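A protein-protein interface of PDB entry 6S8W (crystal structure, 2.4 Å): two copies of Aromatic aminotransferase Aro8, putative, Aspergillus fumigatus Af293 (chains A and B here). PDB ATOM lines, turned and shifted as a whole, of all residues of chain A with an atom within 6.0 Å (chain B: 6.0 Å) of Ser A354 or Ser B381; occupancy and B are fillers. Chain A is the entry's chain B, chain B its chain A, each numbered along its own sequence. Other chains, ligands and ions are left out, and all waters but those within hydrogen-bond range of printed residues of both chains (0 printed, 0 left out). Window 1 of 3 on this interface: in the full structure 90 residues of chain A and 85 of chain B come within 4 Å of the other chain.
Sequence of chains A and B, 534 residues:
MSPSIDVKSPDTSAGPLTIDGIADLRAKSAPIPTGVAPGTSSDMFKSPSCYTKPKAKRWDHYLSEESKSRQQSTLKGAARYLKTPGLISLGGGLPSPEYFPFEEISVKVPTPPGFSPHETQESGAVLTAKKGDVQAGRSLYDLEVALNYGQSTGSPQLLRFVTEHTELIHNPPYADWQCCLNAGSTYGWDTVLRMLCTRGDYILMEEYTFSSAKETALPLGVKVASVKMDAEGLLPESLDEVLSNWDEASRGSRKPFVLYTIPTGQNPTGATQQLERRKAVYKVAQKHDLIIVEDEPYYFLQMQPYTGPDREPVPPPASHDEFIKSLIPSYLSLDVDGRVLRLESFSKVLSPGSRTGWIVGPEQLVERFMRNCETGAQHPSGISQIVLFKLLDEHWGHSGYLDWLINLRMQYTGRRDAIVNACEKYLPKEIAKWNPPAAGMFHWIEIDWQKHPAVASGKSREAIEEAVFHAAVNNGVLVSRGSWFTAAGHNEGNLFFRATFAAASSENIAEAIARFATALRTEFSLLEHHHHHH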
ATOM      1  N   PHE A 346     -27.443   4.054  12.784  1.00  0.00           N
ATOM      2  CA  PHE A 346     -26.013   4.085  13.182  1.00  0.00           C
ATOM      3  C   PHE A 346     -25.501   5.527  13.119  1.00  0.00           C
ATOM      4  O   PHE A 346     -24.354   5.779  13.532  1.00  0.00           O
ATOM      5  CB  PHE A 346     -25.190   3.157  12.286  1.00  0.00           C
ATOM      6  CG  PHE A 346     -25.336   1.696  12.622  1.00  0.00           C
ATOM      7  CD1 PHE A 346     -24.929   1.215  13.855  1.00  0.00           C
ATOM      8  CD2 PHE A 346     -25.884   0.805  11.717  1.00  0.00           C
ATOM      9  CE1 PHE A 346     -25.066  -0.127  14.177  1.00  0.00           C
ATOM     10  CE2 PHE A 346     -26.018  -0.537  12.035  1.00  0.00           C
ATOM     11  CZ  PHE A 346     -25.608  -1.001  13.264  1.00  0.00           C
ATOM     12  N   SER A 347     -26.338   6.443  12.624  1.00  0.00           N
ATOM     13  CA  SER A 347     -25.974   7.860  12.364  1.00  0.00           C
ATOM     14  C   SER A 347     -25.422   8.522  13.626  1.00  0.00           C
ATOM     15  O   SER A 347     -24.342   9.107  13.585  1.00  0.00           O
ATOM     16  CB  SER A 347     -27.134   8.627  11.790  1.00  0.00           C
ATOM     17  OG  SER A 347     -27.332   8.289  10.425  1.00  0.00           O
ATOM     18  N   LEU A 350     -22.317   5.794  15.352  1.00  0.00           N
ATOM     19  CA  LEU A 350     -21.039   5.424  14.682  1.00  0.00           C
ATOM     20  C   LEU A 350     -20.741   6.372  13.510  1.00  0.00           C
ATOM     21  O   LEU A 350     -19.602   6.873  13.454  1.00  0.00           O
ATOM     22  CB  LEU A 350     -21.116   3.965  14.221  1.00  0.00           C
ATOM     23  CG  LEU A 350     -21.139   2.915  15.334  1.00  0.00           C
ATOM     24  CD1 LEU A 350     -21.570   1.562  14.791  1.00  0.00           C
ATOM     25  CD2 LEU A 350     -19.783   2.801  16.017  1.00  0.00           C
ATOM     26  N   SER A 351     -21.703   6.609  12.608  1.00  0.00           N
ATOM     27  CA  SER A 351     -21.517   7.473  11.408  1.00  0.00           C
ATOM     28  C   SER A 351     -22.840   7.740  10.693  1.00  0.00           C
ATOM     29  O   SER A 351     -23.521   6.811  10.266  1.00  0.00           O
ATOM     30  CB  SER A 351     -20.514   6.859  10.463  1.00  0.00           C
ATOM     31  N   PRO A 352     -23.233   9.025  10.529  1.00  0.00           N
ATOM     32  CA  PRO A 352     -24.336   9.394   9.642  1.00  0.00           C
ATOM     33  C   PRO A 352     -24.012   9.045   8.181  1.00  0.00           C
ATOM     34  O   PRO A 352     -24.924   8.776   7.420  1.00  0.00           O
ATOM     35  CB  PRO A 352     -24.461  10.918   9.817  1.00  0.00           C
ATOM     36  CG  PRO A 352     -23.784  11.199  11.144  1.00  0.00           C
ATOM     37  CD  PRO A 352     -22.656  10.191  11.214  1.00  0.00           C
ATOM     38  N   GLY A 353     -22.719   9.056   7.841  1.00  0.00           N
ATOM     39  CA  GLY A 353     -22.204   8.814   6.481  1.00  0.00           C
ATOM     40  C   GLY A 353     -22.599   7.444   5.958  1.00  0.00           C
ATOM     41  O   GLY A 353     -22.999   7.351   4.781  1.00  0.00           O
ATOM     42  N   SER A 354     -22.489   6.416   6.805  1.00  0.00           N
ATOM     43  CA  SER A 354     -22.737   4.991   6.461  1.00  0.00           C
ATOM     44  C   SER A 354     -24.144   4.805   5.877  1.00  0.00           C
ATOM     45  O   SER A 354     -24.347   3.810   5.157  1.00  0.00           O
ATOM     46  CB  SER A 354     -22.528   4.102   7.658  1.00  0.00           C
ATOM     47  OG  SER A 354     -23.516   4.344   8.648  1.00  0.00           O
ATOM     48  N   ARG A 355     -25.080   5.709   6.183  1.00  0.00           N
ATOM     49  CA  ARG A 355     -26.490   5.624   5.717  1.00  0.00           C
ATOM     50  C   ARG A 355     -27.014   4.214   5.994  1.00  0.00           C
ATOM     51  O   ARG A 355     -27.524   3.573   5.053  1.00  0.00           O
ATOM     52  CB  ARG A 355     -26.593   5.923   4.218  1.00  0.00           C
ATOM     53  CG  ARG A 355     -26.515   7.399   3.856  1.00  0.00           C
ATOM     54  CD  ARG A 355     -27.713   8.190   4.338  1.00  0.00           C
ATOM     55  NE  ARG A 355     -27.502   8.601   5.715  1.00  0.00           N
ATOM     56  CZ  ARG A 355     -28.468   8.858   6.585  1.00  0.00           C
ATOM     57  NH1 ARG A 355     -29.736   8.745   6.226  1.00  0.00           N
ATOM     58  NH2 ARG A 355     -28.159   9.221   7.815  1.00  0.00           N
ATOM     59  N   THR A 356     -26.876   3.743   7.233  1.00  0.00           N
ATOM     60  CA  THR A 356     -27.268   2.371   7.643  1.00  0.00           C
ATOM     61  C   THR A 356     -28.056   2.435   8.946  1.00  0.00           C
ATOM     62  O   THR A 356     -27.573   3.064   9.906  1.00  0.00           O
ATOM     63  CB  THR A 356     -26.041   1.456   7.748  1.00  0.00           C
ATOM     64  OG1 THR A 356     -26.498   0.115   7.923  1.00  0.00           O
ATOM     65  N   PRO A 380     -28.926  -1.140   2.483  1.00  0.00           N
ATOM     66  CA  PRO A 380     -27.837  -0.205   2.717  1.00  0.00           C
ATOM     67  C   PRO A 380     -26.592  -0.712   1.973  1.00  0.00           C
ATOM     68  O   PRO A 380     -26.424  -1.914   1.881  1.00  0.00           O
ATOM     69  CB  PRO A 380     -27.612  -0.264   4.233  1.00  0.00           C
ATOM     70  CG  PRO A 380     -28.219  -1.572   4.663  1.00  0.00           C
ATOM     71  CD  PRO A 380     -29.345  -1.839   3.690  1.00  0.00           C
ATOM     72  N   SER A 381     -25.694   0.205   1.585  1.00  0.00           N
ATOM     73  CA  SER A 381     -24.446  -0.064   0.826  1.00  0.00           C
ATOM     74  C   SER A 381     -23.727  -1.280   1.414  1.00  0.00           C
ATOM     75  O   SER A 381     -23.558  -1.334   2.650  1.00  0.00           O
ATOM     76  CB  SER A 381     -23.558   1.153   0.810  1.00  0.00           C
ATOM     77  OG  SER A 381     -22.189   0.782   0.883  1.00  0.00           O
ATOM     78  N   ILE A 383     -20.541  -2.094   1.116  1.00  0.00           N
ATOM     79  CA  ILE A 383     -19.248  -1.690   1.747  1.00  0.00           C
ATOM     80  C   ILE A 383     -19.529  -1.158   3.157  1.00  0.00           C
ATOM     81  O   ILE A 383     -18.747  -1.454   4.060  1.00  0.00           O
ATOM     82  CB  ILE A 383     -18.422  -0.741   0.859  1.00  0.00           C
ATOM     83  CG1 ILE A 383     -18.358   0.681   1.413  1.00  0.00           C
ATOM     84  CG2 ILE A 383     -18.907  -0.780  -0.578  1.00  0.00           C
ATOM     85  CD1 ILE A 383     -17.191   1.475   0.891  1.00  0.00           C
ATOM     86  N   SER A 384     -20.610  -0.396   3.315  1.00  0.00           N
ATOM     87  CA  SER A 384     -21.081   0.074   4.645  1.00  0.00           C
ATOM     88  C   SER A 384     -21.296  -1.137   5.560  1.00  0.00           C
ATOM     89  O   SER A 384     -20.789  -1.117   6.698  1.00  0.00           O
ATOM     90  CB  SER A 384     -22.335   0.905   4.537  1.00  0.00           C
ATOM     91  OG  SER A 384     -22.026   2.291   4.542  1.00  0.00           O
ATOM     92  N   LEU A 388     -19.104  -2.205   9.042  1.00  0.00           N
ATOM     93  CA  LEU A 388     -19.859  -2.233  10.325  1.00  0.00           C
ATOM     94  C   LEU A 388     -19.753  -3.630  10.947  1.00  0.00           C
ATOM     95  O   LEU A 388     -19.539  -3.709  12.172  1.00  0.00           O
ATOM     96  CB  LEU A 388     -21.322  -1.846  10.080  1.00  0.00           C
ATOM     97  CG  LEU A 388     -21.583  -0.355   9.868  1.00  0.00           C
ATOM     98  CD1 LEU A 388     -23.027  -0.107   9.465  1.00  0.00           C
ATOM     99  CD2 LEU A 388     -21.238   0.443  11.118  1.00  0.00           C
ATOM    100  N   ALA B 146     -16.921  12.479   4.658  1.00  0.00           N
ATOM    101  CA  ALA B 146     -17.514  11.236   4.108  1.00  0.00           C
ATOM    102  C   ALA B 146     -18.384  10.553   5.170  1.00  0.00           C
ATOM    103  O   ALA B 146     -19.495  10.101   4.825  1.00  0.00           O
ATOM    104  CB  ALA B 146     -16.423  10.309   3.630  1.00  0.00           C
ATOM    105  N   LEU B 147     -17.887  10.483   6.408  1.00  0.00           N
ATOM    106  CA  LEU B 147     -18.507   9.724   7.530  1.00  0.00           C
ATOM    107  C   LEU B 147     -19.626  10.537   8.180  1.00  0.00           C
ATOM    108  O   LEU B 147     -20.359   9.961   9.008  1.00  0.00           O
ATOM    109  CB  LEU B 147     -17.431   9.390   8.564  1.00  0.00           C
ATOM    110  CG  LEU B 147     -16.354   8.422   8.085  1.00  0.00           C
ATOM    111  CD1 LEU B 147     -15.265   8.272   9.134  1.00  0.00           C
ATOM    112  CD2 LEU B 147     -16.960   7.073   7.734  1.00  0.00           C
ATOM    113  N   ASN B 148     -19.749  11.819   7.837  1.00  0.00           N
ATOM    114  CA  ASN B 148     -20.801  12.690   8.417  1.00  0.00           C
ATOM    115  C   ASN B 148     -21.962  12.772   7.428  1.00  0.00           C
ATOM    116  O   ASN B 148     -21.898  12.110   6.374  1.00  0.00           O
ATOM    117  CB  ASN B 148     -20.272  14.079   8.783  1.00  0.00           C
ATOM    118  CG  ASN B 148     -20.924  14.639  10.030  1.00  0.00           C
ATOM    119  OD1 ASN B 148     -22.147  14.665  10.139  1.00  0.00           O
ATOM    120  ND2 ASN B 148     -20.112  15.086  10.979  1.00  0.00           N
ATOM    121  N   SER B 354     -22.169  -1.288  -3.900  1.00  0.00           N
ATOM    122  CA  SER B 354     -21.853   0.126  -3.585  1.00  0.00           C
ATOM    123  C   SER B 354     -23.140   0.908  -3.323  1.00  0.00           C
ATOM    124  O   SER B 354     -23.073   1.928  -2.632  1.00  0.00           O
ATOM    125  CB  SER B 354     -21.064   0.747  -4.702  1.00  0.00           C
ATOM    126  OG  SER B 354     -21.747   0.602  -5.934  1.00  0.00           O
ATOM    127  N   ARG B 355     -24.259   0.461  -3.900  1.00  0.00           N
ATOM    128  CA  ARG B 355     -25.568   1.156  -3.768  1.00  0.00           C
ATOM    129  C   ARG B 355     -25.374   2.628  -4.140  1.00  0.00           C
ATOM    130  O   ARG B 355     -25.812   3.491  -3.374  1.00  0.00           O
ATOM    131  CB  ARG B 355     -26.147   1.013  -2.355  1.00  0.00           C
ATOM    132  CG  ARG B 355     -26.687  -0.371  -2.026  1.00  0.00           C
ATOM    133  CD  ARG B 355     -27.812  -0.831  -2.930  1.00  0.00           C
ATOM    134  NE  ARG B 355     -27.301  -1.297  -4.205  1.00  0.00           N
ATOM    135  CZ  ARG B 355     -27.937  -1.194  -5.361  1.00  0.00           C
ATOM    136  NH1 ARG B 355     -29.135  -0.645  -5.414  1.00  0.00           N
ATOM    137  NH2 ARG B 355     -27.375  -1.647  -6.461  1.00  0.00           N
ATOM    138  N   HIS B 379     -28.775  10.381   0.668  1.00  0.00           N
ATOM    139  CA  HIS B 379     -27.601  10.372  -0.243  1.00  0.00           C
ATOM    140  C   HIS B 379     -26.969   8.983  -0.228  1.00  0.00           C
ATOM    141  O   HIS B 379     -27.250   8.225   0.705  1.00  0.00           O
ATOM    142  CB  HIS B 379     -26.591  11.462   0.139  1.00  0.00           C
ATOM    143  CG  HIS B 379     -26.075  11.350   1.532  1.00  0.00           C
ATOM    144  ND1 HIS B 379     -26.578  12.100   2.565  1.00  0.00           N
ATOM    145  CD2 HIS B 379     -25.112  10.579   2.069  1.00  0.00           C
ATOM    146  CE1 HIS B 379     -25.951  11.792   3.676  1.00  0.00           C
ATOM    147  NE2 HIS B 379     -25.049  10.862   3.397  1.00  0.00           N
ATOM    148  N   PRO B 380     -26.144   8.612  -1.225  1.00  0.00           N
ATOM    149  CA  PRO B 380     -25.481   7.320  -1.216  1.00  0.00           C
ATOM    150  C   PRO B 380     -24.467   7.282  -0.065  1.00  0.00           C
ATOM    151  O   PRO B 380     -23.858   8.285   0.209  1.00  0.00           O
ATOM    152  CB  PRO B 380     -24.721   7.276  -2.545  1.00  0.00           C
ATOM    153  CG  PRO B 380     -25.342   8.359  -3.387  1.00  0.00           C
ATOM    154  CD  PRO B 380     -25.831   9.401  -2.408  1.00  0.00           C
ATOM    155  N   SER B 381     -24.325   6.124   0.576  1.00  0.00           N
ATOM    156  CA  SER B 381     -23.340   5.929   1.673  1.00  0.00           C
ATOM    157  C   SER B 381     -22.087   6.770   1.394  1.00  0.00           C
ATOM    158  O   SER B 381     -21.527   6.652   0.289  1.00  0.00           O
ATOM    159  CB  SER B 381     -22.997   4.473   1.857  1.00  0.00           C
ATOM    160  OG  SER B 381     -21.727   4.326   2.474  1.00  0.00           O
ATOM    161  N   GLY B 382     -21.681   7.589   2.369  1.00  0.00           N
ATOM    162  CA  GLY B 382     -20.469   8.428   2.303  1.00  0.00           C
ATOM    163  C   GLY B 382     -19.223   7.576   2.165  1.00  0.00           C
ATOM    164  O   GLY B 382     -18.261   8.032   1.520  1.00  0.00           O
ATOM    165  N   ILE B 383     -19.246   6.375   2.757  1.00  0.00           N
ATOM    166  CA  ILE B 383     -18.145   5.370   2.672  1.00  0.00           C
ATOM    167  C   ILE B 383     -18.068   4.852   1.232  1.00  0.00           C
ATOM    168  O   ILE B 383     -16.940   4.677   0.730  1.00  0.00           O
ATOM    169  CB  ILE B 383     -18.354   4.235   3.695  1.00  0.00           C
ATOM    170  CG1 ILE B 383     -18.349   4.772   5.128  1.00  0.00           C
ATOM    171  CG2 ILE B 383     -17.320   3.137   3.500  1.00  0.00           C
ATOM    172  CD1 ILE B 383     -18.688   3.740   6.176  1.00  0.00           C
ATOM    173  N   SER B 384     -19.220   4.624   0.593  1.00  0.00           N
ATOM    174  CA  SER B 384     -19.325   4.266  -0.845  1.00  0.00           C
ATOM    175  C   SER B 384     -18.736   5.395  -1.699  1.00  0.00           C
ATOM    176  O   SER B 384     -18.005   5.086  -2.661  1.00  0.00           O
ATOM    177  CB  SER B 384     -20.750   3.973  -1.243  1.00  0.00           C
ATOM    178  OG  SER B 384     -21.116   2.649  -0.882  1.00  0.00           O
ATOM    179  N   GLN B 385     -19.036   6.650  -1.349  1.00  0.00           N
ATOM    180  CA  GLN B 385     -18.689   7.845  -2.164  1.00  0.00           C
ATOM    181  C   GLN B 385     -17.178   8.107  -2.111  1.00  0.00           C
ATOM    182  O   GLN B 385     -16.597   8.329  -3.190  1.00  0.00           O
ATOM    183  CB  GLN B 385     -19.481   9.072  -1.713  1.00  0.00           C
ATOM    184  CG  GLN B 385     -20.926   9.060  -2.188  1.00  0.00           C
ATOM    185  CD  GLN B 385     -21.578  10.416  -2.085  1.00  0.00           C
ATOM    186  OE1 GLN B 385     -20.978  11.442  -2.399  1.00  0.00           O
ATOM    187  NE2 GLN B 385     -22.825  10.430  -1.645  1.00  0.00           N
ATOM    188  N   ILE B 386     -16.560   8.093  -0.924  1.00  0.00           N
ATOM    189  CA  ILE B 386     -15.112   8.434  -0.778  1.00  0.00           C
ATOM    190  C   ILE B 386     -14.275   7.353  -1.473  1.00  0.00           C
ATOM    191  O   ILE B 386     -13.207   7.697  -2.017  1.00  0.00           O
ATOM    192  CB  ILE B 386     -14.686   8.644   0.687  1.00  0.00           C
ATOM    193  CG1 ILE B 386     -13.346   9.384   0.752  1.00  0.00           C
ATOM    194  CG2 ILE B 386     -14.644   7.331   1.460  1.00  0.00           C
ATOM    195  CD1 ILE B 386     -13.082  10.089   2.060  1.00  0.00           C
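Of the 14 printed residues of chain A, 8 touch a printed residue of chain B. Hydrophobic or aromatic side chains of chain B within 4 Å of the printed part of chain A: His B379 and Ile B383. Along chain B the printed residues that touch a printed residue of chain A span positions 146 to 384. Among the printed residues, 18 pairs touch across the chains.
Among the printed residues, pairs that only touch across the chains: Ile A383 with Ile B383 (3.1 Å), Arg A355 with His B379 (3.3 Å), Gly A353 with Ala B146 (3.4 Å), Ser A351 with Leu B147 (3.4 Å), Gly A353 with Ser B381 (3.4 Å), Ser A381 with Ser B381 (3.5 Å), Ser A381 with Ser B354 (3.6 Å), Ser A354 with Ser B381 (3.6 Å), Ser A381 with Arg B355 (3.6 Å), Ile A383 with Ser B384 (3.8 Å), Pro A352 with Asn B148 (3.9 Å) and Ser A384 with Ile B383 (3.99 Å).
The backbone carbonyl oxygen (O) of Leu B147 lies within hydrogen-bond range of the backbone NH (N) of Gly A353 (2.8 Å). The backbone carbonyl oxygen (O) of Asn B148 lies close to the backbone NH (N) of Gly A353 (3.5 Å). OG of Ser A384 sits at hydrogen-bond distance from OG of Ser B381, 2.9 Å away. The backbone NH (N) of Gly B382 sits at hydrogen-bond distance from the backbone carbonyl oxygen (O) of Gly A353 (2.8 Å). The side-chain hydroxyl (OG) of Ser B384 sits at hydrogen-bond distance from the side-chain hydroxyl (OG) of Ser A381, 2.8 Å away. The backbone nitrogen (N) of Pro A352 lies close to the backbone carbonyl oxygen (O) of Leu B147, 3.4 Å away.
Ser A354 touches one residue of chain B. Ser B381 touches just these residues of chain A: Gly A353, Ser A354, Ser A381 and Ser A384. Of the printed residues of chain B, Gly A353 touches Ala B146, Leu B147, Asn B148, Ser B381 and Gly B382. Printed residues of chain A within 4 Å of Ala B146: Gly A353 (3.4 Å). Printed residues of chain A within 4 Å of Leu B147: Ser A351, Pro A352 and Gly A353. Of the printed residues of chain B, Ile A383 touches Ile B383 and Ser B384. The nearest residue of chain A that does not touch Ser B381 is Arg A355 (4.1 Å). The nearest printed residue of chain B that does not touch Gly A353 is His B379 (4.3 Å).
OG of Ser B381 lies close to N of Ile B383 (3.2 Å). The backbone carbonyl oxygen (O) of Phe A346 sits at hydrogen-bond distance from the backbone NH (N) of Ser A351. O of Pro A352 sits at hydrogen-bond distance from NE of Arg A355 (3.1 Å). The backbone carbonyl oxygen of Ser A354 sits at hydrogen-bond distance from the side-chain hydroxyl of Ser A384. The side-chain hydroxyl (OG) of Ser A381 lies close to the backbone NH (N) of Ile A383. The side-chain hydroxyl of Ser A381 is in hydrogen-bond range of the backbone NH of Ser A384 (3.1 Å).
Ser A381 touches Arg B355, but with the chains exchanged Arg A355 does not touch Ser B381 (4.1 Å). Ser B381 touches its own counterpart, Ser A381. Ile A383 touches its own counterpart, Ile B383. Ile A383 touches Ser B384, and with the chains exchanged Ser A384 touches Ile B383. Positions printed for both chains: 354, 355, 380, 381, 383 and 384. Of the 18 pairs that touch across the chains among the printed residues, 8 have their exchanged pair printed and touching as well.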
